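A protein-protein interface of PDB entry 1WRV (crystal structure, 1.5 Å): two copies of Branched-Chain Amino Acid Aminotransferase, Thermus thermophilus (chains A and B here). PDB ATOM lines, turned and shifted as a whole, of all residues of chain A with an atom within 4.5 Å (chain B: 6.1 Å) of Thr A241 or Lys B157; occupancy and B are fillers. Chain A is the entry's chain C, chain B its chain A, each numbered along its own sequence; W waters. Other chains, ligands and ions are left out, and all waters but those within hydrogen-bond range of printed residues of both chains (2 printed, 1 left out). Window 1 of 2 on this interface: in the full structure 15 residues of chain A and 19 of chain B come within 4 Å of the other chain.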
ATOM      1  N   TYR A 190     -10.360  -6.034   9.203  1.00  0.00           N
ATOM      2  CA  TYR A 190      -9.385  -7.115   9.318  1.00  0.00           C
ATOM      3  C   TYR A 190      -7.974  -6.568   9.219  1.00  0.00           C
ATOM      4  O   TYR A 190      -7.762  -5.469   8.717  1.00  0.00           O
ATOM      5  CB  TYR A 190      -9.574  -8.152   8.210  1.00  0.00           C
ATOM      6  CG  TYR A 190     -10.821  -8.976   8.350  1.00  0.00           C
ATOM      7  CD1 TYR A 190     -11.971  -8.658   7.637  1.00  0.00           C
ATOM      8  CD2 TYR A 190     -10.857 -10.064   9.221  1.00  0.00           C
ATOM      9  CE1 TYR A 190     -13.132  -9.408   7.788  1.00  0.00           C
ATOM     10  CE2 TYR A 190     -12.008 -10.815   9.382  1.00  0.00           C
ATOM     11  CZ  TYR A 190     -13.140 -10.485   8.665  1.00  0.00           C
ATOM     12  OH  TYR A 190     -14.279 -11.235   8.835  1.00  0.00           O
ATOM     13  N   VAL A 191      -7.005  -7.341   9.689  1.00  0.00           N
ATOM     14  CA  VAL A 191      -5.624  -6.900   9.605  1.00  0.00           C
ATOM     15  C   VAL A 191      -5.212  -6.867   8.137  1.00  0.00           C
ATOM     16  O   VAL A 191      -5.564  -7.758   7.362  1.00  0.00           O
ATOM     17  CB  VAL A 191      -4.679  -7.850  10.359  1.00  0.00           C
ATOM     18  CG1 VAL A 191      -3.227  -7.408  10.162  1.00  0.00           C
ATOM     19  CG2 VAL A 191      -5.029  -7.861  11.835  1.00  0.00           C
ATOM     20  N   ALA A 240      -6.889 -12.454   8.941  1.00  0.00           N
ATOM     21  CA  ALA A 240      -6.752 -12.390  10.390  1.00  0.00           C
ATOM     22  C   ALA A 240      -7.305 -11.127  11.017  1.00  0.00           C
ATOM     23  O   ALA A 240      -7.381 -10.078  10.377  1.00  0.00           O
ATOM     24  CB  ALA A 240      -5.280 -12.544  10.771  1.00  0.00           C
ATOM     25  N   THR A 241      -7.689 -11.240  12.284  1.00  0.00           N
ATOM     26  CA  THR A 241      -8.205 -10.103  13.031  1.00  0.00           C
ATOM     27  C   THR A 241      -7.124  -9.666  14.007  1.00  0.00           C
ATOM     28  O   THR A 241      -6.158 -10.394  14.252  1.00  0.00           O
ATOM     29  CB  THR A 241      -9.463 -10.459  13.834  1.00  0.00           C
ATOM     30  OG1 THR A 241      -9.131 -11.417  14.848  1.00  0.00           O
ATOM     31  CG2 THR A 241     -10.528 -11.036  12.912  1.00  0.00           C
ATOM     32  N   ARG A 242      -7.293  -8.479  14.572  1.00  0.00           N
ATOM     33  CA  ARG A 242      -6.306  -7.961  15.506  1.00  0.00           C
ATOM     34  C   ARG A 242      -6.171  -8.853  16.727  1.00  0.00           C
ATOM     35  O   ARG A 242      -5.057  -9.087  17.199  1.00  0.00           O
ATOM     36  CB  ARG A 242      -6.678  -6.537  15.929  1.00  0.00           C
ATOM     37  CG  ARG A 242      -7.981  -6.434  16.710  1.00  0.00           C
ATOM     38  CD  ARG A 242      -8.502  -5.005  16.701  1.00  0.00           C
ATOM     39  NE  ARG A 242      -7.597  -4.063  17.355  1.00  0.00           N
ATOM     40  CZ  ARG A 242      -7.709  -2.743  17.256  1.00  0.00           C
ATOM     41  NH1 ARG A 242      -8.684  -2.211  16.529  1.00  0.00           N
ATOM     42  NH2 ARG A 242      -6.844  -1.953  17.879  1.00  0.00           N
ATOM     43  N   ASP A 243      -7.291  -9.362  17.238  1.00  0.00           N
ATOM     44  CA  ASP A 243      -7.199 -10.211  18.412  1.00  0.00           C
ATOM     45  C   ASP A 243      -6.655 -11.605  18.126  1.00  0.00           C
ATOM     46  O   ASP A 243      -6.278 -12.318  19.049  1.00  0.00           O
ATOM     47  CB  ASP A 243      -8.517 -10.249  19.224  1.00  0.00           C
ATOM     48  CG  ASP A 243      -9.780 -10.319  18.377  1.00  0.00           C
ATOM     49  OD1 ASP A 243      -9.750 -10.103  17.147  1.00  0.00           O
ATOM     50  OD2 ASP A 243     -10.837 -10.581  18.993  1.00  0.00           O
ATOM     51  N   GLN A 244      -6.592 -11.999  16.858  1.00  0.00           N
ATOM     52  CA  GLN A 244      -5.981 -13.284  16.554  1.00  0.00           C
ATOM     53  C   GLN A 244      -4.485 -13.060  16.744  1.00  0.00           C
ATOM     54  O   GLN A 244      -3.762 -13.953  17.176  1.00  0.00           O
ATOM     55  CB  GLN A 244      -6.280 -13.725  15.123  1.00  0.00           C
ATOM     56  CG  GLN A 244      -7.636 -14.389  14.991  1.00  0.00           C
ATOM     57  CD  GLN A 244      -7.953 -14.798  13.573  1.00  0.00           C
ATOM     58  OE1 GLN A 244      -8.091 -13.958  12.693  1.00  0.00           O
ATOM     59  NE2 GLN A 244      -8.076 -16.103  13.346  1.00  0.00           N
ATOM     60  N   LEU A 245      -4.023 -11.853  16.433  1.00  0.00           N
ATOM     61  CA  LEU A 245      -2.613 -11.530  16.610  1.00  0.00           C
ATOM     62  C   LEU A 245      -2.298 -11.406  18.103  1.00  0.00           C
ATOM     63  O   LEU A 245      -1.286 -11.922  18.565  1.00  0.00           O
ATOM     64  CB  LEU A 245      -2.253 -10.223  15.897  1.00  0.00           C
ATOM     65  CG  LEU A 245      -2.471 -10.148  14.381  1.00  0.00           C
ATOM     66  CD1 LEU A 245      -1.785  -8.897  13.835  1.00  0.00           C
ATOM     67  CD2 LEU A 245      -1.914 -11.383  13.711  1.00  0.00           C
ATOM     68  N   MET A 247      -3.450 -12.921  20.531  1.00  0.00           N
ATOM     69  CA  MET A 247      -3.369 -14.254  21.127  1.00  0.00           C
ATOM     70  C   MET A 247      -2.354 -15.195  20.481  1.00  0.00           C
ATOM     71  O   MET A 247      -2.227 -16.350  20.888  1.00  0.00           O
ATOM     72  CB  MET A 247      -4.745 -14.933  21.083  1.00  0.00           C
ATOM     73  CG  MET A 247      -5.863 -14.216  21.827  1.00  0.00           C
ATOM     74  SD  MET A 247      -7.465 -15.028  21.571  1.00  0.00           S
ATOM     75  CE  MET A 247      -8.324 -13.746  20.774  1.00  0.00           C
ATOM     76  N   ARG B  59      -7.749 -19.679  26.557  1.00  0.00           N
ATOM     77  CA  ARG B  59      -8.609 -18.695  25.925  1.00  0.00           C
ATOM     78  C   ARG B  59      -9.167 -17.721  26.957  1.00  0.00           C
ATOM     79  O   ARG B  59      -9.407 -16.556  26.652  1.00  0.00           O
ATOM     80  CB  ARG B  59      -9.748 -19.395  25.174  1.00  0.00           C
ATOM     81  CG  ARG B  59     -10.493 -18.475  24.224  1.00  0.00           C
ATOM     82  CD  ARG B  59     -11.403 -19.269  23.304  1.00  0.00           C
ATOM     83  NE  ARG B  59     -12.493 -19.927  24.023  1.00  0.00           N
ATOM     84  CZ  ARG B  59     -13.325 -20.800  23.465  1.00  0.00           C
ATOM     85  NH1 ARG B  59     -13.181 -21.122  22.184  1.00  0.00           N
ATOM     86  NH2 ARG B  59     -14.304 -21.337  24.175  1.00  0.00           N
ATOM     87  N   SER B  63      -8.667 -13.914  26.433  1.00  0.00           N
ATOM     88  CA  SER B  63      -9.774 -12.962  26.404  1.00  0.00           C
ATOM     89  C   SER B  63      -9.466 -11.787  27.324  1.00  0.00           C
ATOM     90  O   SER B  63      -9.712 -10.631  26.978  1.00  0.00           O
ATOM     91  CB  SER B  63     -11.080 -13.639  26.833  1.00  0.00           C
ATOM     92  OG  SER B  63     -11.518 -14.563  25.847  1.00  0.00           O
ATOM     93  N   VAL B  66      -7.152  -9.217  25.806  1.00  0.00           N
ATOM     94  CA  VAL B  66      -7.780  -8.313  24.852  1.00  0.00           C
ATOM     95  C   VAL B  66      -8.287  -7.065  25.570  1.00  0.00           C
ATOM     96  O   VAL B  66      -8.209  -5.961  25.037  1.00  0.00           O
ATOM     97  CB  VAL B  66      -8.967  -8.988  24.123  1.00  0.00           C
ATOM     98  CG1 VAL B  66      -9.601  -8.014  23.151  1.00  0.00           C
ATOM     99  CG2 VAL B  66      -8.491 -10.206  23.377  1.00  0.00           C
ATOM    100  N   ARG B 148     -23.009  -9.883  13.088  1.00  0.00           N
ATOM    101  CA  ARG B 148     -21.963 -10.063  14.088  1.00  0.00           C
ATOM    102  C   ARG B 148     -20.990  -8.909  13.866  1.00  0.00           C
ATOM    103  O   ARG B 148     -20.712  -8.528  12.732  1.00  0.00           O
ATOM    104  CB  ARG B 148     -21.240 -11.406  13.944  1.00  0.00           C
ATOM    105  CG  ARG B 148     -20.214 -11.616  15.077  1.00  0.00           C
ATOM    106  CD  ARG B 148     -19.748 -13.058  15.204  1.00  0.00           C
ATOM    107  NE  ARG B 148     -18.649 -13.216  16.162  1.00  0.00           N
ATOM    108  CZ  ARG B 148     -18.787 -13.366  17.477  1.00  0.00           C
ATOM    109  NH1 ARG B 148     -19.987 -13.381  18.040  1.00  0.00           N
ATOM    110  NH2 ARG B 148     -17.708 -13.512  18.234  1.00  0.00           N
ATOM    111  N   ALA B 151     -14.425  -6.969  13.042  1.00  0.00           N
ATOM    112  CA  ALA B 151     -13.249  -7.244  13.855  1.00  0.00           C
ATOM    113  C   ALA B 151     -12.584  -6.035  14.500  1.00  0.00           C
ATOM    114  O   ALA B 151     -11.656  -6.191  15.292  1.00  0.00           O
ATOM    115  CB  ALA B 151     -12.236  -8.011  13.027  1.00  0.00           C
ATOM    116  N   MET B 154     -15.824  -4.979  18.007  1.00  0.00           N
ATOM    117  CA  MET B 154     -15.841  -5.748  19.249  1.00  0.00           C
ATOM    118  C   MET B 154     -14.853  -6.887  18.995  1.00  0.00           C
ATOM    119  O   MET B 154     -14.702  -7.337  17.858  1.00  0.00           O
ATOM    120  CB  MET B 154     -17.241  -6.316  19.548  1.00  0.00           C
ATOM    121  CG  MET B 154     -18.339  -5.268  19.802  1.00  0.00           C
ATOM    122  SD  MET B 154     -18.184  -4.344  21.354  1.00  0.00           S
ATOM    123  CE  MET B 154     -19.090  -5.430  22.487  1.00  0.00           C
ATOM    124  N   PRO B 155     -14.158  -7.357  20.043  1.00  0.00           N
ATOM    125  CA  PRO B 155     -13.176  -8.445  19.935  1.00  0.00           C
ATOM    126  C   PRO B 155     -13.863  -9.795  19.766  1.00  0.00           C
ATOM    127  O   PRO B 155     -14.124 -10.495  20.740  1.00  0.00           O
ATOM    128  CB  PRO B 155     -12.411  -8.338  21.248  1.00  0.00           C
ATOM    129  CG  PRO B 155     -13.481  -7.915  22.203  1.00  0.00           C
ATOM    130  CD  PRO B 155     -14.228  -6.851  21.427  1.00  0.00           C
ATOM    131  N   GLY B 156     -14.134 -10.152  18.515  1.00  0.00           N
ATOM    132  CA  GLY B 156     -14.830 -11.390  18.209  1.00  0.00           C
ATOM    133  C   GLY B 156     -14.125 -12.703  18.480  1.00  0.00           C
ATOM    134  O   GLY B 156     -14.742 -13.761  18.376  1.00  0.00           O
ATOM    135  N   LYS B 157     -12.845 -12.652  18.828  1.00  0.00           N
ATOM    136  CA  LYS B 157     -12.098 -13.871  19.115  1.00  0.00           C
ATOM    137  C   LYS B 157     -12.072 -14.112  20.615  1.00  0.00           C
ATOM    138  O   LYS B 157     -11.527 -15.104  21.085  1.00  0.00           O
ATOM    139  CB  LYS B 157     -10.663 -13.750  18.591  1.00  0.00           C
ATOM    140  CG  LYS B 157     -10.574 -13.518  17.088  1.00  0.00           C
ATOM    141  CD  LYS B 157     -10.922 -14.781  16.308  1.00  0.00           C
ATOM    142  CE  LYS B 157     -11.228 -14.461  14.849  1.00  0.00           C
ATOM    143  NZ  LYS B 157     -12.493 -13.683  14.715  1.00  0.00           N
ATOM    144  N   ALA B 158     -12.665 -13.194  21.367  1.00  0.00           N
ATOM    145  CA  ALA B 158     -12.687 -13.316  22.817  1.00  0.00           C
ATOM    146  C   ALA B 158     -14.101 -13.447  23.350  1.00  0.00           C
ATOM    147  O   ALA B 158     -15.054 -12.956  22.743  1.00  0.00           O
ATOM    148  CB  ALA B 158     -12.019 -12.107  23.441  1.00  0.00           C
ATOM    149  N   LYS B 159     -14.238 -14.129  24.486  1.00  0.00           N
ATOM    150  CA  LYS B 159     -15.542 -14.277  25.116  1.00  0.00           C
ATOM    151  C   LYS B 159     -15.690 -13.137  26.118  1.00  0.00           C
ATOM    152  O   LYS B 159     -15.627 -13.339  27.331  1.00  0.00           O
ATOM    153  CB  LYS B 159     -15.663 -15.623  25.836  1.00  0.00           C
ATOM    154  CG  LYS B 159     -16.053 -16.790  24.938  1.00  0.00           C
ATOM    155  CD  LYS B 159     -16.535 -17.964  25.789  1.00  0.00           C
ATOM    156  CE  LYS B 159     -16.817 -19.231  25.000  1.00  0.00           C
ATOM    157  NZ  LYS B 159     -17.629 -18.965  23.816  1.00  0.00           N
ATOM    158  N   ASN B 163     -19.828  -8.400  24.313  1.00  0.00           N
ATOM    159  CA  ASN B 163     -20.067  -8.987  23.000  1.00  0.00           C
ATOM    160  C   ASN B 163     -21.428  -9.656  22.923  1.00  0.00           C
ATOM    161  O   ASN B 163     -22.064  -9.667  21.871  1.00  0.00           O
ATOM    162  CB  ASN B 163     -19.028 -10.070  22.691  1.00  0.00           C
ATOM    163  CG  ASN B 163     -17.646  -9.521  22.423  1.00  0.00           C
ATOM    164  OD1 ASN B 163     -17.380  -8.339  22.610  1.00  0.00           O
ATOM    165  ND2 ASN B 163     -16.748 -10.400  21.984  1.00  0.00           N
ATOM    166  N   HIS B 212     -12.609 -18.394  10.135  1.00  0.00           N
ATOM    167  CA  HIS B 212     -12.786 -17.730  11.412  1.00  0.00           C
ATOM    168  C   HIS B 212     -13.436 -16.356  11.305  1.00  0.00           C
ATOM    169  O   HIS B 212     -14.195 -15.970  12.187  1.00  0.00           O
ATOM    170  CB  HIS B 212     -11.437 -17.617  12.124  1.00  0.00           C
ATOM    171  CG  HIS B 212     -10.965 -18.913  12.701  1.00  0.00           C
ATOM    172  ND1 HIS B 212      -9.649 -19.321  12.663  1.00  0.00           N
ATOM    173  CD2 HIS B 212     -11.647 -19.908  13.314  1.00  0.00           C
ATOM    174  CE1 HIS B 212      -9.543 -20.513  13.221  1.00  0.00           C
ATOM    175  NE2 HIS B 212     -10.742 -20.891  13.625  1.00  0.00           N
ATOM    176  N   SER B 213     -13.153 -15.640  10.215  1.00  0.00           N
ATOM    177  CA  SER B 213     -13.663 -14.288   9.979  1.00  0.00           C
ATOM    178  C   SER B 213     -13.849 -13.520  11.289  1.00  0.00           C
ATOM    179  O   SER B 213     -12.870 -13.298  11.992  1.00  0.00           O
ATOM    180  CB  SER B 213     -14.956 -14.314   9.141  1.00  0.00           C
ATOM    181  OG  SER B 213     -16.074 -14.769   9.859  1.00  0.00           O
ATOM    182  N   VAL B 214     -15.072 -13.117  11.625  1.00  0.00           N
ATOM    183  CA  VAL B 214     -15.311 -12.374  12.870  1.00  0.00           C
ATOM    184  C   VAL B 214     -15.841 -13.262  13.995  1.00  0.00           C
ATOM    185  O   VAL B 214     -16.262 -12.767  15.041  1.00  0.00           O
ATOM    186  CB  VAL B 214     -16.338 -11.235  12.663  1.00  0.00           C
ATOM    187  CG1 VAL B 214     -15.737 -10.130  11.804  1.00  0.00           C
ATOM    188  CG2 VAL B 214     -17.608 -11.791  12.022  1.00  0.00           C
ATOM    189  N   ASN B 215     -15.796 -14.571  13.780  1.00  0.00           N
ATOM    190  CA  ASN B 215     -16.313 -15.536  14.747  1.00  0.00           C
ATOM    191  C   ASN B 215     -15.312 -15.946  15.816  1.00  0.00           C
ATOM    192  O   ASN B 215     -14.115 -15.669  15.715  1.00  0.00           O
ATOM    193  CB  ASN B 215     -16.786 -16.795  14.013  1.00  0.00           C
ATOM    194  CG  ASN B 215     -17.613 -16.478  12.784  1.00  0.00           C
ATOM    195  OD1 ASN B 215     -18.474 -15.601  12.816  1.00  0.00           O
ATOM    196  ND2 ASN B 215     -17.360 -17.198  11.696  1.00  0.00           N
ATOM    197  N   LEU B 216     -15.806 -16.617  16.850  1.00  0.00           N
ATOM    198  CA  LEU B 216     -14.924 -17.083  17.905  1.00  0.00           C
ATOM    199  C   LEU B 216     -14.312 -18.373  17.381  1.00  0.00           C
ATOM    200  O   LEU B 216     -14.974 -19.117  16.663  1.00  0.00           O
ATOM    201  CB  LEU B 216     -15.707 -17.385  19.182  1.00  0.00           C
ATOM    202  CG  LEU B 216     -14.810 -17.550  20.412  1.00  0.00           C
ATOM    203  CD1 LEU B 216     -14.578 -16.186  21.034  1.00  0.00           C
ATOM    204  CD2 LEU B 216     -15.453 -18.475  21.418  1.00  0.00           C
ATOM    205  N   GLU B 217     -13.052 -18.625  17.722  1.00  0.00           N
ATOM    206  CA  GLU B 217     -12.377 -19.841  17.289  1.00  0.00           C
ATOM    207  C   GLU B 217     -12.813 -20.959  18.220  1.00  0.00           C
ATOM    208  O   GLU B 217     -12.181 -21.214  19.240  1.00  0.00           O
ATOM    209  CB  GLU B 217     -10.859 -19.670  17.365  1.00  0.00           C
ATOM    210  CG  GLU B 217     -10.309 -18.579  16.463  1.00  0.00           C
ATOM    211  CD  GLU B 217      -8.795 -18.481  16.527  1.00  0.00           C
ATOM    212  OE1 GLU B 217      -8.218 -17.726  15.722  1.00  0.00           O
ATOM    213  OE2 GLU B 217      -8.180 -19.156  17.383  1.00  0.00           O
HETATM  214  O   HOH W   1     -10.286 -14.143  10.761  1.00  0.00           O
HETATM  215  O   HOH W   2      -9.233  -6.644  13.701  1.00  0.00           O
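The backbone NH of Gly B156 is in hydrogen-bond range of the side-chain carboxylate of Asp A243 (3.4 Å). The side-chain carboxylate (OD2) of Asp A243 sits at hydrogen-bond distance from the backbone NH (N) of Lys B157 (2.9 Å). The side-chain hydroxyl (OH) of Tyr A190 is in hydrogen-bond range of the backbone NH (N) of Val B214 (3.5 Å). The side-chain carboxylate (OE1) of Glu B217 is in hydrogen-bond range of the side-chain amide nitrogen (NE2) of Gln A244, 2.9 Å away.
NH2 of Arg B148 is in hydrogen-bond range of O of Gly B156 (3.0 Å). The backbone carbonyl oxygen (O) of Gly B156 lies close to the backbone NH (N) of Leu B216 (3.4 Å). NZ of Lys B157 is in hydrogen-bond range of O of Ser B213 (2.8 Å). O of His B212 lies close to ND2 of Asn B215 (3.4 Å). OD1 of Asp A243 sits at hydrogen-bond distance from OG1 of Thr A241 (2.7 Å). OE1 of Gln A244 sits at hydrogen-bond distance from N of Thr A241 (2.8 Å).
Tyr A190 touches Ser B213. CB of Ala B151 touches CG2 of Thr A241, 3.5 Å away. OG1 of Thr A241 touches CG of Lys B157, at 3.4 Å. Thr A241 touches Ser B213 (CG2 to O, 3.4 Å). Arg A242 touches Ala B151. Pro B155 touches Asp A243 (C to OD2, 3.2 Å). Asp A243 touches Ala B158. Gln A244 touches Lys B157. His B212 touches Gln A244 (ND1 to NE2, 3.6 Å). Met A247 touches Lys B157.
Thr A241 touches three residues of chain B. Of the printed residues of chain A, Ala B158 touches Asp A243. Printed residues of chain B within 4 Å of Tyr A190: Ser B213 (3.2 Å) and Val B214 (3.5 Å). Of the printed residues of chain A, Ala B151 touches Thr A241 and Arg A242. Of the printed residues of chain A, Ser B213 touches Tyr A190 (3.2 Å) and Thr A241 (3.4 Å). Arg B148 touches none of the printed residues of chain A. Val A191 touches none of the printed residues of chain B. The nearest printed residue of chain A that does not touch Lys B157 is Tyr A190 (6.1 Å). The nearest printed residue of chain A that does not touch Glu B217 is Met A247 (5.9 Å).
Of the 9 printed residues of chain A, 6 touch a printed residue of chain B. Hydrophobic or aromatic side chains of chain A within 4 Å of the printed part of chain B: Tyr A190 and Met A247. Of the 18 printed residues of chain B, 9 touch a printed residue of chain A. Printed residues of chain B that touch a printed residue of chain A: Ala B151, Pro B155, Gly B156, Lys B157, Ala B158, His B212, Ser B213, Val B214 and Glu B217. Among the printed residues, 14 pairs touch across the chains.
No position is printed for both chains. Of the 14 pairs that touch across the chains among the printed residues, none has its exchanged pair printed and touching as well.
Water W2 lies within hydrogen-bond range of N of Arg A242 (2.8 Å) and O of Ala B151 (2.9 Å). Water W1 bridges OE1 of Gln A244 (2.9 Å) and O of Ser B213 (3.0 Å).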
